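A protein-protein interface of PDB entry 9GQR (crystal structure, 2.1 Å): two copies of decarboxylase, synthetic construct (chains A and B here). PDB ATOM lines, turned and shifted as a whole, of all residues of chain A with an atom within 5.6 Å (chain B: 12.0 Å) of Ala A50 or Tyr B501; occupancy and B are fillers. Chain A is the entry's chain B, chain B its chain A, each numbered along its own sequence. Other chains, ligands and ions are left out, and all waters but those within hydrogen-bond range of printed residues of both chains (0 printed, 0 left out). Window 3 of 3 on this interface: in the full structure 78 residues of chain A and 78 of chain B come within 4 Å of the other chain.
Among the printed residues, pairs that only touch across the chains: Ile A24 with Tyr B499 (3.2 Å), Ile A24 with Gly B500 (3.4 Å), Ile A26 with Tyr B499 (3.6 Å), Ile A39 with Val B492 (3.8 Å), Ile A39 with Trp B496 (3.8 Å), Ile A39 with Tyr B499 (3.5 Å), Val A43 with Trp B496 (3.8 Å), Val A43 with Tyr B501 (3.4 Å), Leu A48 with Trp B496 (3.5 Å), Leu A48 with Tyr B501 (3.9 Å) and Ala A50 with Tyr B501 (3.6 Å).
The side-chain hydroxyl of Tyr B501 is in hydrogen-bond range of the backbone carbonyl oxygen of Pro A49, at 2.6 Å.
The side-chain hydroxyl (OH) of Tyr B501 sits close to the backbone nitrogen (N) of Pro A51, 3.3 Å away.
Hydrophobic or aromatic side chains of chain B within 4 Å of the printed part of chain A: Val B492, Trp B496, Tyr B499 and Tyr B501.
No residue of chain B comes within 4 Å of Leu A23.
Of chain B, only Trp B496 and Tyr B501 come within 4 Å of Val A43.
Of chain B, only Trp B496 (3.5 Å) and Tyr B501 (3.9 Å) come within 4 Å of Leu A48.
Of chain B, only Tyr B501 comes within 4 Å of Pro A49.
Of chain B, only Tyr B501 (3.6 Å) comes within 4 Å of Ala A50.
Pro A51 touches one residue of chain B.
No residue of chain B comes within 4 Å of Leu A52.
Of the printed residues of chain A, Trp B496 touches Ile A39 (3.8 Å), Val A43 (3.8 Å) and Leu A48 (3.5 Å).
Of the printed residues of chain A, Gly B500 touches Ile A24 (3.4 Å).
Of the printed residues of chain A, Tyr B501 touches Val A43, Leu A48, Pro A49, Ala A50 and Pro A51.
The nearest residue of chain B that does not touch Ala A50 is Trp B496 (8.5 Å).
No position is printed for both chains.
N of Tyr B501 lies within hydrogen-bond range of O of Trp B496 (3.3 Å).
The backbone NH (N) of Ala A50 lies within hydrogen-bond range of the backbone carbonyl oxygen (O) of Asp A22, at 3.0 Å.
N of Ile A24 lies within hydrogen-bond range of O of Ala A50, at 3.1 Å.
The backbone carbonyl oxygen (O) of Ile A24 sits at hydrogen-bond distance from the backbone NH (N) of Leu A52.
O of Val A43 sits at hydrogen-bond distance from N of Leu A48, at 3.0 Å.
The backbone carbonyl oxygen (O) of Leu A48 is in hydrogen-bond range of the guanidinium group (NH2) of Arg A83.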
ATOM      1  N   LEU A  17     -20.889  20.530 -16.744  1.00  0.00           N
ATOM      2  CA  LEU A  17     -20.069  21.103 -17.807  1.00  0.00           C
ATOM      3  C   LEU A  17     -20.932  21.834 -18.827  1.00  0.00           C
ATOM      4  O   LEU A  17     -20.577  22.926 -19.285  1.00  0.00           O
ATOM      5  CB  LEU A  17     -19.246  20.011 -18.490  1.00  0.00           C
ATOM      6  CG  LEU A  17     -18.190  19.291 -17.650  1.00  0.00           C
ATOM      7  CD1 LEU A  17     -17.430  18.282 -18.498  1.00  0.00           C
ATOM      8  CD2 LEU A  17     -17.236  20.291 -17.019  1.00  0.00           C
ATOM      9  N   ASP A  22     -19.165  24.705 -20.644  1.00  0.00           N
ATOM     10  CA  ASP A  22     -17.896  24.007 -20.823  1.00  0.00           C
ATOM     11  C   ASP A  22     -18.046  22.731 -21.647  1.00  0.00           C
ATOM     12  O   ASP A  22     -17.228  21.816 -21.520  1.00  0.00           O
ATOM     13  CB  ASP A  22     -17.276  23.689 -19.461  1.00  0.00           C
ATOM     14  CG  ASP A  22     -15.777  23.489 -19.533  1.00  0.00           C
ATOM     15  OD1 ASP A  22     -15.166  23.917 -20.530  1.00  0.00           O
ATOM     16  OD2 ASP A  22     -15.212  22.898 -18.591  1.00  0.00           O
ATOM     17  N   LEU A  23     -19.070  22.653 -22.494  1.00  0.00           N
ATOM     18  CA  LEU A  23     -19.310  21.449 -23.278  1.00  0.00           C
ATOM     19  C   LEU A  23     -19.937  21.831 -24.609  1.00  0.00           C
ATOM     20  O   LEU A  23     -20.917  22.581 -24.641  1.00  0.00           O
ATOM     21  CB  LEU A  23     -20.227  20.477 -22.527  1.00  0.00           C
ATOM     22  CG  LEU A  23     -20.455  19.116 -23.189  1.00  0.00           C
ATOM     23  CD1 LEU A  23     -19.477  18.091 -22.640  1.00  0.00           C
ATOM     24  CD2 LEU A  23     -21.896  18.645 -23.013  1.00  0.00           C
ATOM     25  N   ILE A  24     -19.375  21.315 -25.697  1.00  0.00           N
ATOM     26  CA  ILE A  24     -19.942  21.475 -27.032  1.00  0.00           C
ATOM     27  C   ILE A  24     -20.391  20.100 -27.505  1.00  0.00           C
ATOM     28  O   ILE A  24     -19.577  19.174 -27.614  1.00  0.00           O
ATOM     29  CB  ILE A  24     -18.940  22.111 -28.014  1.00  0.00           C
ATOM     30  CG1 ILE A  24     -19.029  23.639 -27.972  1.00  0.00           C
ATOM     31  CG2 ILE A  24     -19.209  21.643 -29.439  1.00  0.00           C
ATOM     32  CD1 ILE A  24     -18.577  24.267 -26.685  1.00  0.00           C
ATOM     33  N   ILE A  26     -21.269  17.827 -30.265  1.00  0.00           N
ATOM     34  CA  ILE A  26     -20.930  17.816 -31.682  1.00  0.00           C
ATOM     35  C   ILE A  26     -21.825  16.805 -32.389  1.00  0.00           C
ATOM     36  O   ILE A  26     -21.688  15.594 -32.190  1.00  0.00           O
ATOM     37  CB  ILE A  26     -19.448  17.493 -31.898  1.00  0.00           C
ATOM     38  CG1 ILE A  26     -18.575  18.460 -31.099  1.00  0.00           C
ATOM     39  CG2 ILE A  26     -19.100  17.555 -33.377  1.00  0.00           C
ATOM     40  CD1 ILE A  26     -17.088  18.211 -31.255  1.00  0.00           C
ATOM     41  N   ILE A  39      -8.990  16.716 -32.452  1.00  0.00           N
ATOM     42  CA  ILE A  39      -9.914  17.664 -31.835  1.00  0.00           C
ATOM     43  C   ILE A  39      -9.609  17.806 -30.348  1.00  0.00           C
ATOM     44  O   ILE A  39      -9.552  18.919 -29.810  1.00  0.00           O
ATOM     45  CB  ILE A  39     -11.372  17.228 -32.072  1.00  0.00           C
ATOM     46  CG1 ILE A  39     -11.726  17.319 -33.558  1.00  0.00           C
ATOM     47  CG2 ILE A  39     -12.328  18.076 -31.247  1.00  0.00           C
ATOM     48  CD1 ILE A  39     -13.033  16.643 -33.908  1.00  0.00           C
ATOM     49  N   VAL A  43      -8.373  21.062 -28.106  1.00  0.00           N
ATOM     50  CA  VAL A  43      -9.155  21.488 -26.950  1.00  0.00           C
ATOM     51  C   VAL A  43      -8.287  21.515 -25.696  1.00  0.00           C
ATOM     52  O   VAL A  43      -8.413  22.417 -24.859  1.00  0.00           O
ATOM     53  CB  VAL A  43     -10.388  20.581 -26.779  1.00  0.00           C
ATOM     54  CG1 VAL A  43     -11.086  20.866 -25.460  1.00  0.00           C
ATOM     55  CG2 VAL A  43     -11.351  20.784 -27.939  1.00  0.00           C
ATOM     56  N   LEU A  48     -10.154  24.811 -24.311  1.00  0.00           N
ATOM     57  CA  LEU A  48     -11.498  25.055 -24.814  1.00  0.00           C
ATOM     58  C   LEU A  48     -12.495  24.148 -24.110  1.00  0.00           C
ATOM     59  O   LEU A  48     -12.118  23.224 -23.383  1.00  0.00           O
ATOM     60  CB  LEU A  48     -11.514  24.832 -26.326  1.00  0.00           C
ATOM     61  CG  LEU A  48     -10.569  25.732 -27.125  1.00  0.00           C
ATOM     62  CD1 LEU A  48     -10.504  25.292 -28.574  1.00  0.00           C
ATOM     63  CD2 LEU A  48     -11.004  27.187 -27.027  1.00  0.00           C
ATOM     64  N   PRO A  49     -13.796  24.398 -24.281  1.00  0.00           N
ATOM     65  CA  PRO A  49     -14.795  23.496 -23.697  1.00  0.00           C
ATOM     66  C   PRO A  49     -14.645  22.069 -24.208  1.00  0.00           C
ATOM     67  O   PRO A  49     -14.233  21.828 -25.346  1.00  0.00           O
ATOM     68  CB  PRO A  49     -16.127  24.111 -24.137  1.00  0.00           C
ATOM     69  CG  PRO A  49     -15.830  25.556 -24.282  1.00  0.00           C
ATOM     70  CD  PRO A  49     -14.415  25.635 -24.795  1.00  0.00           C
ATOM     71  N   ALA A  50     -14.993  21.120 -23.345  1.00  0.00           N
ATOM     72  CA  ALA A  50     -14.795  19.713 -23.658  1.00  0.00           C
ATOM     73  C   ALA A  50     -15.754  19.267 -24.760  1.00  0.00           C
ATOM     74  O   ALA A  50     -16.936  19.624 -24.743  1.00  0.00           O
ATOM     75  CB  ALA A  50     -15.002  18.857 -22.409  1.00  0.00           C
ATOM     76  N   PRO A  51     -15.277  18.490 -25.732  1.00  0.00           N
ATOM     77  CA  PRO A  51     -16.158  18.032 -26.811  1.00  0.00           C
ATOM     78  C   PRO A  51     -16.928  16.778 -26.428  1.00  0.00           C
ATOM     79  O   PRO A  51     -16.406  15.877 -25.765  1.00  0.00           O
ATOM     80  CB  PRO A  51     -15.182  17.750 -27.959  1.00  0.00           C
ATOM     81  CG  PRO A  51     -13.922  17.342 -27.264  1.00  0.00           C
ATOM     82  CD  PRO A  51     -13.866  18.142 -25.981  1.00  0.00           C
ATOM     83  N   LEU A  52     -18.187  16.728 -26.856  1.00  0.00           N
ATOM     84  CA  LEU A  52     -19.039  15.550 -26.699  1.00  0.00           C
ATOM     85  C   LEU A  52     -19.420  15.074 -28.096  1.00  0.00           C
ATOM     86  O   LEU A  52     -20.320  15.635 -28.729  1.00  0.00           O
ATOM     87  CB  LEU A  52     -20.274  15.861 -25.860  1.00  0.00           C
ATOM     88  CG  LEU A  52     -21.230  14.682 -25.665  1.00  0.00           C
ATOM     89  CD1 LEU A  52     -20.518  13.516 -24.992  1.00  0.00           C
ATOM     90  CD2 LEU A  52     -22.455  15.098 -24.868  1.00  0.00           C
ATOM     91  N   LEU A  67     -16.882  11.401 -24.737  1.00  0.00           N
ATOM     92  CA  LEU A  67     -16.647  12.630 -23.988  1.00  0.00           C
ATOM     93  C   LEU A  67     -15.145  12.869 -23.972  1.00  0.00           C
ATOM     94  O   LEU A  67     -14.392  12.098 -23.363  1.00  0.00           O
ATOM     95  CB  LEU A  67     -17.199  12.542 -22.566  1.00  0.00           C
ATOM     96  CG  LEU A  67     -16.776  13.741 -21.710  1.00  0.00           C
ATOM     97  CD1 LEU A  67     -17.452  15.019 -22.192  1.00  0.00           C
ATOM     98  CD2 LEU A  67     -17.040  13.510 -20.230  1.00  0.00           C
ATOM     99  N   GLY A  68     -14.709  13.929 -24.646  1.00  0.00           N
ATOM    100  CA  GLY A  68     -13.303  14.250 -24.748  1.00  0.00           C
ATOM    101  C   GLY A  68     -12.864  15.251 -23.700  1.00  0.00           C
ATOM    102  O   GLY A  68     -13.657  16.047 -23.201  1.00  0.00           O
ATOM    103  N   CYS A  69     -11.575  15.191 -23.370  1.00  0.00           N
ATOM    104  CA  CYS A  69     -10.941  16.094 -22.416  1.00  0.00           C
ATOM    105  C   CYS A  69     -11.704  16.216 -21.090  1.00  0.00           C
ATOM    106  O   CYS A  69     -12.025  17.321 -20.655  1.00  0.00           O
ATOM    107  CB  CYS A  69     -10.759  17.469 -23.042  1.00  0.00           C
ATOM    108  SG  CYS A  69     -10.090  17.434 -24.720  1.00  0.00           S
ATOM    109  N   PRO A  70     -11.998  15.093 -20.420  1.00  0.00           N
ATOM    110  CA  PRO A  70     -12.729  15.191 -19.147  1.00  0.00           C
ATOM    111  C   PRO A  70     -11.929  15.850 -18.038  1.00  0.00           C
ATOM    112  O   PRO A  70     -12.532  16.346 -17.078  1.00  0.00           O
ATOM    113  CB  PRO A  70     -13.049  13.730 -18.811  1.00  0.00           C
ATOM    114  CG  PRO A  70     -11.954  12.959 -19.463  1.00  0.00           C
ATOM    115  CD  PRO A  70     -11.643  13.697 -20.736  1.00  0.00           C
ATOM    116  N   ARG A  83     -12.787  21.142 -14.142  1.00  0.00           N
ATOM    117  CA  ARG A  83     -13.139  19.757 -14.437  1.00  0.00           C
ATOM    118  C   ARG A  83     -12.521  18.794 -13.433  1.00  0.00           C
ATOM    119  O   ARG A  83     -13.079  17.719 -13.180  1.00  0.00           O
ATOM    120  CB  ARG A  83     -12.706  19.394 -15.857  1.00  0.00           C
ATOM    121  CG  ARG A  83     -13.430  20.176 -16.940  1.00  0.00           C
ATOM    122  CD  ARG A  83     -12.882  19.850 -18.318  1.00  0.00           C
ATOM    123  NE  ARG A  83     -13.068  20.963 -19.241  1.00  0.00           N
ATOM    124  CZ  ARG A  83     -12.545  21.024 -20.458  1.00  0.00           C
ATOM    125  NH1 ARG A  83     -11.806  20.041 -20.943  1.00  0.00           N
ATOM    126  NH2 ARG A  83     -12.768  22.102 -21.206  1.00  0.00           N
ATOM    127  N   PHE B 481      -1.511  18.944 -31.360  1.00  0.00           N
ATOM    128  CA  PHE B 481      -2.338  19.115 -32.552  1.00  0.00           C
ATOM    129  C   PHE B 481      -1.486  19.205 -33.811  1.00  0.00           C
ATOM    130  O   PHE B 481      -1.804  18.579 -34.830  1.00  0.00           O
ATOM    131  CB  PHE B 481      -3.221  20.357 -32.422  1.00  0.00           C
ATOM    132  CG  PHE B 481      -4.021  20.656 -33.661  1.00  0.00           C
ATOM    133  CD1 PHE B 481      -5.218  20.000 -33.906  1.00  0.00           C
ATOM    134  CD2 PHE B 481      -3.572  21.587 -34.587  1.00  0.00           C
ATOM    135  CE1 PHE B 481      -5.956  20.268 -35.048  1.00  0.00           C
ATOM    136  CE2 PHE B 481      -4.302  21.858 -35.730  1.00  0.00           C
ATOM    137  CZ  PHE B 481      -5.495  21.197 -35.961  1.00  0.00           C
ATOM    138  N   LYS B 491      -8.760  19.105 -41.894  1.00  0.00           N
ATOM    139  CA  LYS B 491     -10.163  18.729 -41.744  1.00  0.00           C
ATOM    140  C   LYS B 491     -10.752  19.294 -40.457  1.00  0.00           C
ATOM    141  O   LYS B 491     -11.875  19.812 -40.459  1.00  0.00           O
ATOM    142  CB  LYS B 491     -10.305  17.207 -41.778  1.00  0.00           C
ATOM    143  CG  LYS B 491     -11.745  16.715 -41.809  1.00  0.00           C
ATOM    144  CD  LYS B 491     -12.449  17.147 -43.086  1.00  0.00           C
ATOM    145  CE  LYS B 491     -13.847  16.557 -43.173  1.00  0.00           C
ATOM    146  NZ  LYS B 491     -14.554  16.983 -44.411  1.00  0.00           N
ATOM    147  N   VAL B 492     -10.007  19.212 -39.352  1.00  0.00           N
ATOM    148  CA  VAL B 492     -10.517  19.682 -38.067  1.00  0.00           C
ATOM    149  C   VAL B 492     -10.670  21.200 -38.063  1.00  0.00           C
ATOM    150  O   VAL B 492     -11.674  21.732 -37.570  1.00  0.00           O
ATOM    151  CB  VAL B 492      -9.603  19.196 -36.928  1.00  0.00           C
ATOM    152  CG1 VAL B 492      -9.937  19.909 -35.631  1.00  0.00           C
ATOM    153  CG2 VAL B 492      -9.731  17.690 -36.760  1.00  0.00           C
ATOM    154  N   LEU B 493      -9.686  21.920 -38.607  1.00  0.00           N
ATOM    155  CA  LEU B 493      -9.777  23.376 -38.654  1.00  0.00           C
ATOM    156  C   LEU B 493     -10.913  23.830 -39.561  1.00  0.00           C
ATOM    157  O   LEU B 493     -11.570  24.838 -39.280  1.00  0.00           O
ATOM    158  CB  LEU B 493      -8.448  23.968 -39.121  1.00  0.00           C
ATOM    159  CG  LEU B 493      -7.244  23.751 -38.203  1.00  0.00           C
ATOM    160  CD1 LEU B 493      -5.940  23.985 -38.951  1.00  0.00           C
ATOM    161  CD2 LEU B 493      -7.329  24.649 -36.978  1.00  0.00           C
ATOM    162  N   GLN B 494     -11.163  23.100 -40.649  1.00  0.00           N
ATOM    163  CA  GLN B 494     -12.247  23.471 -41.553  1.00  0.00           C
ATOM    164  C   GLN B 494     -13.607  23.309 -40.889  1.00  0.00           C
ATOM    165  O   GLN B 494     -14.519  24.113 -41.122  1.00  0.00           O
ATOM    166  CB  GLN B 494     -12.172  22.634 -42.830  1.00  0.00           C
ATOM    167  CG  GLN B 494     -11.161  23.125 -43.852  1.00  0.00           C
ATOM    168  CD  GLN B 494     -11.111  22.241 -45.083  1.00  0.00           C
ATOM    169  OE1 GLN B 494     -11.581  21.105 -45.061  1.00  0.00           O
ATOM    170  NE2 GLN B 494     -10.546  22.763 -46.167  1.00  0.00           N
ATOM    171  N   ASN B 495     -13.760  22.286 -40.054  1.00  0.00           N
ATOM    172  CA  ASN B 495     -15.024  21.989 -39.393  1.00  0.00           C
ATOM    173  C   ASN B 495     -15.085  22.511 -37.960  1.00  0.00           C
ATOM    174  O   ASN B 495     -16.003  22.141 -37.218  1.00  0.00           O
ATOM    175  CB  ASN B 495     -15.277  20.481 -39.403  1.00  0.00           C
ATOM    176  CG  ASN B 495     -15.332  19.906 -40.802  1.00  0.00           C
ATOM    177  OD1 ASN B 495     -14.583  18.987 -41.138  1.00  0.00           O
ATOM    178  ND2 ASN B 495     -16.222  20.443 -41.628  1.00  0.00           N
ATOM    179  N   TRP B 496     -14.138  23.361 -37.556  1.00  0.00           N
ATOM    180  CA  TRP B 496     -14.084  23.785 -36.160  1.00  0.00           C
ATOM    181  C   TRP B 496     -15.335  24.560 -35.765  1.00  0.00           C
ATOM    182  O   TRP B 496     -15.857  24.386 -34.658  1.00  0.00           O
ATOM    183  CB  TRP B 496     -12.831  24.621 -35.908  1.00  0.00           C
ATOM    184  CG  TRP B 496     -12.476  24.689 -34.460  1.00  0.00           C
ATOM    185  CD1 TRP B 496     -12.476  25.796 -33.666  1.00  0.00           C
ATOM    186  CD2 TRP B 496     -12.093  23.593 -33.623  1.00  0.00           C
ATOM    187  NE1 TRP B 496     -12.105  25.458 -32.386  1.00  0.00           N
ATOM    188  CE2 TRP B 496     -11.867  24.110 -32.335  1.00  0.00           C
ATOM    189  CE3 TRP B 496     -11.916  22.223 -33.841  1.00  0.00           C
ATOM    190  CZ2 TRP B 496     -11.471  23.309 -31.269  1.00  0.00           C
ATOM    191  CZ3 TRP B 496     -11.522  21.429 -32.782  1.00  0.00           C
ATOM    192  CH2 TRP B 496     -11.304  21.975 -31.511  1.00  0.00           C
ATOM    193  N   SER B 497     -15.831  25.420 -36.656  1.00  0.00           N
ATOM    194  CA  SER B 497     -17.072  26.131 -36.378  1.00  0.00           C
ATOM    195  C   SER B 497     -18.284  25.218 -36.515  1.00  0.00           C
ATOM    196  O   SER B 497     -19.253  25.357 -35.762  1.00  0.00           O
ATOM    197  CB  SER B 497     -17.206  27.337 -37.307  1.00  0.00           C
ATOM    198  OG  SER B 497     -18.509  27.885 -37.230  1.00  0.00           O
ATOM    199  N   ALA B 498     -18.246  24.282 -37.469  1.00  0.00           N
ATOM    200  CA  ALA B 498     -19.345  23.334 -37.620  1.00  0.00           C
ATOM    201  C   ALA B 498     -19.464  22.414 -36.412  1.00  0.00           C
ATOM    202  O   ALA B 498     -20.567  21.955 -36.093  1.00  0.00           O
ATOM    203  CB  ALA B 498     -19.163  22.515 -38.897  1.00  0.00           C
ATOM    204  N   TYR B 499     -18.348  22.131 -35.734  1.00  0.00           N
ATOM    205  CA  TYR B 499     -18.407  21.354 -34.501  1.00  0.00           C
ATOM    206  C   TYR B 499     -19.197  22.083 -33.423  1.00  0.00           C
ATOM    207  O   TYR B 499     -19.866  21.442 -32.604  1.00  0.00           O
ATOM    208  CB  TYR B 499     -16.997  21.055 -33.992  1.00  0.00           C
ATOM    209  CG  TYR B 499     -16.166  20.172 -34.894  1.00  0.00           C
ATOM    210  CD1 TYR B 499     -16.765  19.250 -35.744  1.00  0.00           C
ATOM    211  CD2 TYR B 499     -14.778  20.259 -34.892  1.00  0.00           C
ATOM    212  CE1 TYR B 499     -16.003  18.440 -36.569  1.00  0.00           C
ATOM    213  CE2 TYR B 499     -14.009  19.458 -35.713  1.00  0.00           C
ATOM    214  CZ  TYR B 499     -14.626  18.549 -36.548  1.00  0.00           C
ATOM    215  OH  TYR B 499     -13.860  17.749 -37.365  1.00  0.00           O
ATOM    216  N   GLY B 500     -19.134  23.411 -33.405  1.00  0.00           N
ATOM    217  CA  GLY B 500     -19.766  24.212 -32.372  1.00  0.00           C
ATOM    218  C   GLY B 500     -18.818  25.119 -31.615  1.00  0.00           C
ATOM    219  O   GLY B 500     -19.251  25.774 -30.656  1.00  0.00           O
ATOM    220  N   TYR B 501     -17.546  25.192 -31.992  1.00  0.00           N
ATOM    221  CA  TYR B 501     -16.585  26.040 -31.307  1.00  0.00           C
ATOM    222  C   TYR B 501     -16.514  27.413 -31.965  1.00  0.00           C
ATOM    223  O   TYR B 501     -16.681  27.553 -33.180  1.00  0.00           O
ATOM    224  CB  TYR B 501     -15.199  25.393 -31.301  1.00  0.00           C
ATOM    225  CG  TYR B 501     -15.082  24.214 -30.363  1.00  0.00           C
ATOM    226  CD1 TYR B 501     -14.714  24.396 -29.035  1.00  0.00           C
ATOM    227  CD2 TYR B 501     -15.344  22.919 -30.801  1.00  0.00           C
ATOM    228  CE1 TYR B 501     -14.608  23.325 -28.171  1.00  0.00           C
ATOM    229  CE2 TYR B 501     -15.239  21.840 -29.943  1.00  0.00           C
ATOM    230  CZ  TYR B 501     -14.871  22.050 -28.630  1.00  0.00           C
ATOM    231  OH  TYR B 501     -14.766  20.982 -27.769  1.00  0.00           O
ATOM    232  N   LYS B 502     -16.258  28.427 -31.145  1.00  0.00           N
ATOM    233  CA  LYS B 502     -16.166  29.804 -31.616  1.00  0.00           C
ATOM    234  C   LYS B 502     -14.916  30.027 -32.462  1.00  0.00           C
ATOM    235  O   LYS B 502     -14.004  29.199 -32.471  1.00  0.00           O
ATOM    236  CB  LYS B 502     -16.185  30.772 -30.430  1.00  0.00           C
ATOM    237  CG  LYS B 502     -17.577  31.017 -29.865  1.00  0.00           C
ATOM    238  CD  LYS B 502     -17.538  31.761 -28.539  1.00  0.00           C
ATOM    239  CE  LYS B 502     -17.396  30.802 -27.367  1.00  0.00           C
ATOM    240  NZ  LYS B 502     -17.996  31.357 -26.120  1.00  0.00           N
